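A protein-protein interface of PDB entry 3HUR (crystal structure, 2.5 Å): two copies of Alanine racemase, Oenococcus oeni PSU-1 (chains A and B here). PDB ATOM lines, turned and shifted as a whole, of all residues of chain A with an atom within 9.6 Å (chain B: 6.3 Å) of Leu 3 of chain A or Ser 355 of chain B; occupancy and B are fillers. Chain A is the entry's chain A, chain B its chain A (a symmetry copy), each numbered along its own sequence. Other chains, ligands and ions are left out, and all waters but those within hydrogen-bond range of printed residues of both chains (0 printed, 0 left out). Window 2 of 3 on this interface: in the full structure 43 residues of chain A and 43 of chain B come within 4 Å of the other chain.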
ATOM      1  N   LEU A   3     -22.608  29.542 -12.465  1.00  0.00           N
ATOM      2  CA  LEU A   3     -22.132  28.449 -13.376  1.00  0.00           C
ATOM      3  C   LEU A   3     -20.662  28.180 -13.060  1.00  0.00           C
ATOM      4  O   LEU A   3     -19.905  29.131 -12.899  1.00  0.00           O
ATOM      5  CB  LEU A   3     -22.278  28.885 -14.840  1.00  0.00           C
ATOM      6  CG  LEU A   3     -22.122  27.865 -15.992  1.00  0.00           C
ATOM      7  CD1 LEU A   3     -23.193  26.789 -15.932  1.00  0.00           C
ATOM      8  CD2 LEU A   3     -22.203  28.537 -17.376  1.00  0.00           C
ATOM      9  N   THR A   4     -20.239  26.922 -12.938  1.00  0.00           N
ATOM     10  CA  THR A   4     -18.854  26.684 -12.505  1.00  0.00           C
ATOM     11  C   THR A   4     -17.970  25.925 -13.508  1.00  0.00           C
ATOM     12  O   THR A   4     -18.416  25.049 -14.215  1.00  0.00           O
ATOM     13  CB  THR A   4     -18.781  26.102 -11.079  1.00  0.00           C
ATOM     14  OG1 THR A   4     -17.767  25.087 -11.024  1.00  0.00           O
ATOM     15  CG2 THR A   4     -20.151  25.560 -10.607  1.00  0.00           C
ATOM     16  N   ALA A   5     -16.722  26.344 -13.606  1.00  0.00           N
ATOM     17  CA  ALA A   5     -15.773  25.813 -14.572  1.00  0.00           C
ATOM     18  C   ALA A   5     -14.743  24.960 -13.825  1.00  0.00           C
ATOM     19  O   ALA A   5     -14.127  25.414 -12.858  1.00  0.00           O
ATOM     20  CB  ALA A   5     -15.080  26.929 -15.297  1.00  0.00           C
ATOM     21  N   ILE A   6     -14.572  23.729 -14.279  1.00  0.00           N
ATOM     22  CA  ILE A   6     -13.675  22.804 -13.657  1.00  0.00           C
ATOM     23  C   ILE A   6     -12.524  22.653 -14.643  1.00  0.00           C
ATOM     24  O   ILE A   6     -12.658  22.010 -15.692  1.00  0.00           O
ATOM     25  CB  ILE A   6     -14.397  21.454 -13.368  1.00  0.00           C
ATOM     26  CG1 ILE A   6     -15.601  21.711 -12.458  1.00  0.00           C
ATOM     27  CG2 ILE A   6     -13.427  20.405 -12.734  1.00  0.00           C
ATOM     28  CD1 ILE A   6     -16.462  20.537 -12.203  1.00  0.00           C
ATOM     29  N   ALA A 258     -19.061  16.651 -11.218  1.00  0.00           N
ATOM     30  CA  ALA A 258     -19.299  17.637 -12.282  1.00  0.00           C
ATOM     31  C   ALA A 258     -20.786  17.840 -12.613  1.00  0.00           C
ATOM     32  O   ALA A 258     -21.162  18.860 -13.178  1.00  0.00           O
ATOM     33  CB  ALA A 258     -18.522  17.253 -13.581  1.00  0.00           C
ATOM     34  N   ASP A 259     -21.619  16.858 -12.265  1.00  0.00           N
ATOM     35  CA  ASP A 259     -23.040  16.921 -12.552  1.00  0.00           C
ATOM     36  C   ASP A 259     -23.811  16.000 -11.594  1.00  0.00           C
ATOM     37  O   ASP A 259     -23.393  14.870 -11.334  1.00  0.00           O
ATOM     38  CB  ASP A 259     -23.268  16.508 -14.009  1.00  0.00           C
ATOM     39  CG  ASP A 259     -24.681  16.850 -14.534  1.00  0.00           C
ATOM     40  OD1 ASP A 259     -25.258  17.856 -14.069  1.00  0.00           O
ATOM     41  OD2 ASP A 259     -25.185  16.112 -15.441  1.00  0.00           O
ATOM     42  N   VAL A 260     -24.924  16.503 -11.062  1.00  0.00           N
ATOM     43  CA  VAL A 260     -25.886  15.697 -10.277  1.00  0.00           C
ATOM     44  C   VAL A 260     -27.289  15.745 -10.911  1.00  0.00           C
ATOM     45  O   VAL A 260     -27.804  16.822 -11.213  1.00  0.00           O
ATOM     46  CB  VAL A 260     -26.026  16.192  -8.840  1.00  0.00           C
ATOM     47  CG1 VAL A 260     -26.742  15.139  -8.005  1.00  0.00           C
ATOM     48  CG2 VAL A 260     -24.665  16.500  -8.248  1.00  0.00           C
ATOM     49  N   ARG A 261     -27.865  14.560 -11.118  1.00  0.00           N
ATOM     50  CA  ARG A 261     -29.179  14.380 -11.718  1.00  0.00           C
ATOM     51  C   ARG A 261     -30.058  13.522 -10.787  1.00  0.00           C
ATOM     52  O   ARG A 261     -29.623  12.466 -10.313  1.00  0.00           O
ATOM     53  CB  ARG A 261     -29.036  13.641 -13.046  1.00  0.00           C
ATOM     54  CG  ARG A 261     -28.435  14.449 -14.240  1.00  0.00           C
ATOM     55  CD  ARG A 261     -28.295  13.543 -15.471  1.00  0.00           C
ATOM     56  NE  ARG A 261     -27.353  12.463 -15.196  1.00  0.00           N
ATOM     57  CZ  ARG A 261     -27.289  11.278 -15.814  1.00  0.00           C
ATOM     58  NH1 ARG A 261     -28.128  10.930 -16.790  1.00  0.00           N
ATOM     59  NH2 ARG A 261     -26.356  10.401 -15.423  1.00  0.00           N
ATOM     60  N   THR A 285     -22.178  12.416 -11.945  1.00  0.00           N
ATOM     61  CA  THR A 285     -21.241  12.200 -13.062  1.00  0.00           C
ATOM     62  C   THR A 285     -19.845  12.770 -12.705  1.00  0.00           C
ATOM     63  O   THR A 285     -19.717  13.958 -12.355  1.00  0.00           O
ATOM     64  CB  THR A 285     -21.691  12.985 -14.281  1.00  0.00           C
ATOM     65  OG1 THR A 285     -23.011  12.597 -14.588  1.00  0.00           O
ATOM     66  CG2 THR A 285     -20.773  12.764 -15.505  1.00  0.00           C
ATOM     67  N   ILE A 331     -22.210  20.165  -6.606  1.00  0.00           N
ATOM     68  CA  ILE A 331     -21.155  19.969  -7.561  1.00  0.00           C
ATOM     69  C   ILE A 331     -19.894  20.485  -6.903  1.00  0.00           C
ATOM     70  O   ILE A 331     -19.945  21.355  -6.054  1.00  0.00           O
ATOM     71  CB  ILE A 331     -21.461  20.624  -8.953  1.00  0.00           C
ATOM     72  CG1 ILE A 331     -21.445  22.133  -8.869  1.00  0.00           C
ATOM     73  CG2 ILE A 331     -22.800  20.113  -9.552  1.00  0.00           C
ATOM     74  CD1 ILE A 331     -20.221  22.718  -9.495  1.00  0.00           C
ATOM     75  N   TRP B  90     -14.031  32.884 -10.180  1.00  0.00           N
ATOM     76  CA  TRP B  90     -14.705  34.102  -9.824  1.00  0.00           C
ATOM     77  C   TRP B  90     -15.553  33.959  -8.577  1.00  0.00           C
ATOM     78  O   TRP B  90     -16.531  34.671  -8.429  1.00  0.00           O
ATOM     79  CB  TRP B  90     -15.552  34.607 -11.015  1.00  0.00           C
ATOM     80  CG  TRP B  90     -16.466  33.602 -11.551  1.00  0.00           C
ATOM     81  CD1 TRP B  90     -17.562  33.099 -10.931  1.00  0.00           C
ATOM     82  CD2 TRP B  90     -16.386  32.956 -12.820  1.00  0.00           C
ATOM     83  NE1 TRP B  90     -18.165  32.155 -11.736  1.00  0.00           N
ATOM     84  CE2 TRP B  90     -17.461  32.058 -12.903  1.00  0.00           C
ATOM     85  CE3 TRP B  90     -15.499  33.034 -13.885  1.00  0.00           C
ATOM     86  CZ2 TRP B  90     -17.683  31.250 -14.013  1.00  0.00           C
ATOM     87  CZ3 TRP B  90     -15.703  32.224 -14.993  1.00  0.00           C
ATOM     88  CH2 TRP B  90     -16.786  31.338 -15.047  1.00  0.00           C
ATOM     89  N   PRO B 108     -18.445  36.748 -15.414  1.00  0.00           N
ATOM     90  CA  PRO B 108     -19.117  35.675 -16.098  1.00  0.00           C
ATOM     91  C   PRO B 108     -20.536  35.979 -16.530  1.00  0.00           C
ATOM     92  O   PRO B 108     -21.043  35.309 -17.439  1.00  0.00           O
ATOM     93  CB  PRO B 108     -19.134  34.575 -15.032  1.00  0.00           C
ATOM     94  CG  PRO B 108     -19.310  35.316 -13.796  1.00  0.00           C
ATOM     95  CD  PRO B 108     -18.444  36.532 -13.962  1.00  0.00           C
ATOM     96  N   ARG B 135     -20.397  29.437 -23.016  1.00  0.00           N
ATOM     97  CA  ARG B 135     -21.473  29.814 -22.090  1.00  0.00           C
ATOM     98  C   ARG B 135     -21.020  30.865 -21.082  1.00  0.00           C
ATOM     99  O   ARG B 135     -21.773  31.259 -20.203  1.00  0.00           O
ATOM    100  CB  ARG B 135     -21.992  28.577 -21.382  1.00  0.00           C
ATOM    101  CG  ARG B 135     -22.406  27.466 -22.343  1.00  0.00           C
ATOM    102  CD  ARG B 135     -22.524  26.125 -21.659  1.00  0.00           C
ATOM    103  NE  ARG B 135     -23.444  26.172 -20.525  1.00  0.00           N
ATOM    104  CZ  ARG B 135     -23.625  25.177 -19.660  1.00  0.00           C
ATOM    105  NH1 ARG B 135     -22.955  24.032 -19.793  1.00  0.00           N
ATOM    106  NH2 ARG B 135     -24.471  25.337 -18.648  1.00  0.00           N
ATOM    107  N   ILE B 136     -19.787  31.333 -21.233  1.00  0.00           N
ATOM    108  CA  ILE B 136     -19.208  32.267 -20.302  1.00  0.00           C
ATOM    109  C   ILE B 136     -19.430  33.686 -20.830  1.00  0.00           C
ATOM    110  O   ILE B 136     -19.155  33.985 -22.013  1.00  0.00           O
ATOM    111  CB  ILE B 136     -17.675  32.033 -20.111  1.00  0.00           C
ATOM    112  CG1 ILE B 136     -17.312  30.530 -20.012  1.00  0.00           C
ATOM    113  CG2 ILE B 136     -17.196  32.765 -18.870  1.00  0.00           C
ATOM    114  CD1 ILE B 136     -15.720  30.222 -19.902  1.00  0.00           C
ATOM    115  N   ASN B 353     -19.822  19.584 -21.295  1.00  0.00           N
ATOM    116  CA  ASN B 353     -20.781  20.583 -20.834  1.00  0.00           C
ATOM    117  C   ASN B 353     -21.901  19.908 -20.092  1.00  0.00           C
ATOM    118  O   ASN B 353     -22.465  18.931 -20.566  1.00  0.00           O
ATOM    119  CB  ASN B 353     -21.311  21.449 -22.000  1.00  0.00           C
ATOM    120  CG  ASN B 353     -20.298  22.510 -22.434  1.00  0.00           C
ATOM    121  OD1 ASN B 353     -20.333  23.647 -21.947  1.00  0.00           O
ATOM    122  ND2 ASN B 353     -19.368  22.133 -23.335  1.00  0.00           N
ATOM    123  N   TYR B 354     -22.199  20.432 -18.923  1.00  0.00           N
ATOM    124  CA  TYR B 354     -23.289  19.937 -18.110  1.00  0.00           C
ATOM    125  C   TYR B 354     -24.153  21.111 -17.636  1.00  0.00           C
ATOM    126  O   TYR B 354     -23.813  22.275 -17.818  1.00  0.00           O
ATOM    127  CB  TYR B 354     -22.755  19.150 -16.890  1.00  0.00           C
ATOM    128  CG  TYR B 354     -21.915  17.983 -17.276  1.00  0.00           C
ATOM    129  CD1 TYR B 354     -22.511  16.824 -17.706  1.00  0.00           C
ATOM    130  CD2 TYR B 354     -20.513  18.041 -17.248  1.00  0.00           C
ATOM    131  CE1 TYR B 354     -21.744  15.728 -18.088  1.00  0.00           C
ATOM    132  CE2 TYR B 354     -19.743  16.935 -17.608  1.00  0.00           C
ATOM    133  CZ  TYR B 354     -20.366  15.804 -18.046  1.00  0.00           C
ATOM    134  OH  TYR B 354     -19.698  14.702 -18.448  1.00  0.00           O
ATOM    135  N   SER B 355     -25.266  20.778 -17.007  1.00  0.00           N
ATOM    136  CA  SER B 355     -26.249  21.751 -16.627  1.00  0.00           C
ATOM    137  C   SER B 355     -25.616  22.971 -15.945  1.00  0.00           C
ATOM    138  O   SER B 355     -25.789  24.088 -16.394  1.00  0.00           O
ATOM    139  CB  SER B 355     -27.268  21.082 -15.715  1.00  0.00           C
ATOM    140  OG  SER B 355     -28.274  22.012 -15.378  1.00  0.00           O
ATOM    141  N   HIS B 356     -24.843  22.744 -14.892  1.00  0.00           N
ATOM    142  CA  HIS B 356     -24.270  23.837 -14.084  1.00  0.00           C
ATOM    143  C   HIS B 356     -22.721  23.964 -14.135  1.00  0.00           C
ATOM    144  O   HIS B 356     -22.134  24.778 -13.402  1.00  0.00           O
ATOM    145  CB  HIS B 356     -24.736  23.679 -12.620  1.00  0.00           C
ATOM    146  CG  HIS B 356     -26.211  23.908 -12.415  1.00  0.00           C
ATOM    147  ND1 HIS B 356     -27.068  22.916 -11.970  1.00  0.00           N
ATOM    148  CD2 HIS B 356     -26.982  25.017 -12.596  1.00  0.00           C
ATOM    149  CE1 HIS B 356     -28.297  23.406 -11.881  1.00  0.00           C
ATOM    150  NE2 HIS B 356     -28.272  24.678 -12.249  1.00  0.00           N
ATOM    151  N   THR B 357     -22.063  23.205 -15.012  1.00  0.00           N
ATOM    152  CA  THR B 357     -20.620  23.115 -14.970  1.00  0.00           C
ATOM    153  C   THR B 357     -20.034  22.875 -16.367  1.00  0.00           C
ATOM    154  O   THR B 357     -20.680  22.295 -17.199  1.00  0.00           O
ATOM    155  CB  THR B 357     -20.211  22.046 -13.916  1.00  0.00           C
ATOM    156  OG1 THR B 357     -19.635  20.895 -14.526  1.00  0.00           O
ATOM    157  CG2 THR B 357     -21.421  21.608 -13.138  1.00  0.00           C
ATOM    158  N   ILE B 358     -18.841  23.392 -16.619  1.00  0.00           N
ATOM    159  CA  ILE B 358     -18.128  23.201 -17.872  1.00  0.00           C
ATOM    160  C   ILE B 358     -16.797  22.619 -17.474  1.00  0.00           C
ATOM    161  O   ILE B 358     -16.106  23.213 -16.662  1.00  0.00           O
ATOM    162  CB  ILE B 358     -17.779  24.524 -18.556  1.00  0.00           C
ATOM    163  CG1 ILE B 358     -19.024  25.355 -18.828  1.00  0.00           C
ATOM    164  CG2 ILE B 358     -16.962  24.298 -19.834  1.00  0.00           C
ATOM    165  CD1 ILE B 358     -18.722  26.860 -18.965  1.00  0.00           C
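The backbone carbonyl oxygen (O) of Ala 258 of chain A sits close to the side-chain hydroxyl (OG1) of Thr 357 of chain B, 2.9 Å away. The backbone carbonyl oxygen (O) of Ile 358 of chain B is in hydrogen-bond range of the backbone NH (N) of Ile 6 of chain A, 2.9 Å away. O of His 356 of chain B sits at hydrogen-bond distance from N of Thr 4 of chain A, at 2.9 Å. The backbone carbonyl oxygen (O) of Thr 4 of chain A is in hydrogen-bond range of the backbone NH (N) of Ile 358 of chain B (3.0 Å).
The guanidinium group of Arg 135 of chain B sits at hydrogen-bond distance from the backbone carbonyl oxygen of Tyr 354 of chain B. The side-chain amide oxygen (OD1) of Asn 353 of chain B sits close to the guanidinium group (NH1) of Arg 135 of chain B (3.4 Å). N of Ala 258 of chain A lies within hydrogen-bond range of O of Thr 285 of chain A (3.0 Å). The guanidinium group (NH2) of Arg 135 of chain B lies within hydrogen-bond range of the backbone carbonyl oxygen (O) of Ser 355 of chain B (2.9 Å). The backbone NH (N) of Thr 285 of chain A sits at hydrogen-bond distance from the backbone carbonyl oxygen (O) of Asp 259 of chain A, 2.8 Å away.
Leu 3 of chain A touches Trp 90 of chain B. NH2 of Arg 135 of chain B touches CD1 of Leu 3 of chain A (3.3 Å). Leu 3 of chain A touches Ser 355 of chain B (CD1 to O, 3.8 Å). Leu 3 of chain A touches His 356 of chain B (CD1 to C, 3.4 Å). Thr 357 of chain B touches Leu 3 of chain A. Ile 358 of chain B touches Ala 5 of chain A (O to CA, 3.4 Å). CD1 of Ile 6 of chain A touches OG1 of Thr 357 of chain B (3.9 Å). Asp 259 of chain A touches Tyr 354 of chain B (OD2 to CD1, 3.6 Å). Tyr 354 of chain B touches Thr 285 of chain A. Ile 331 of chain A touches Thr 357 of chain B (CD1 to CG2, 3.99 Å).
Leu 3 of chain A touches just these residues of chain B: Trp 90, Arg 135, Ser 355, His 356 and Thr 357. Of chain A, only Leu 3 (3.8 Å) comes within 4 Å of Ser 355 of chain B. Of the printed residues of chain A, His 356 of chain B touches Leu 3 and Thr 4. Printed residues of chain B within 4 Å of Ala 258 of chain A: Thr 357 (2.8 Å). Of the printed residues of chain A, Trp 90 of chain B touches Leu 3. Of the printed residues of chain B, Asp 259 of chain A touches Tyr 354. Of the printed residues of chain B, Ile 331 of chain A touches Thr 357 (3.99 Å). The nearest printed residue of chain B that does not touch Thr 285 of chain A is Thr 357 of chain B (7.3 Å).
Of the 10 printed residues of chain A, 8 touch a printed residue of chain B. Hydrophobic or aromatic side chains of chain A that line the printed part of chain B: Leu 3, Ile 6, Ala 258 and Ile 331.
No position is printed for both chains.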
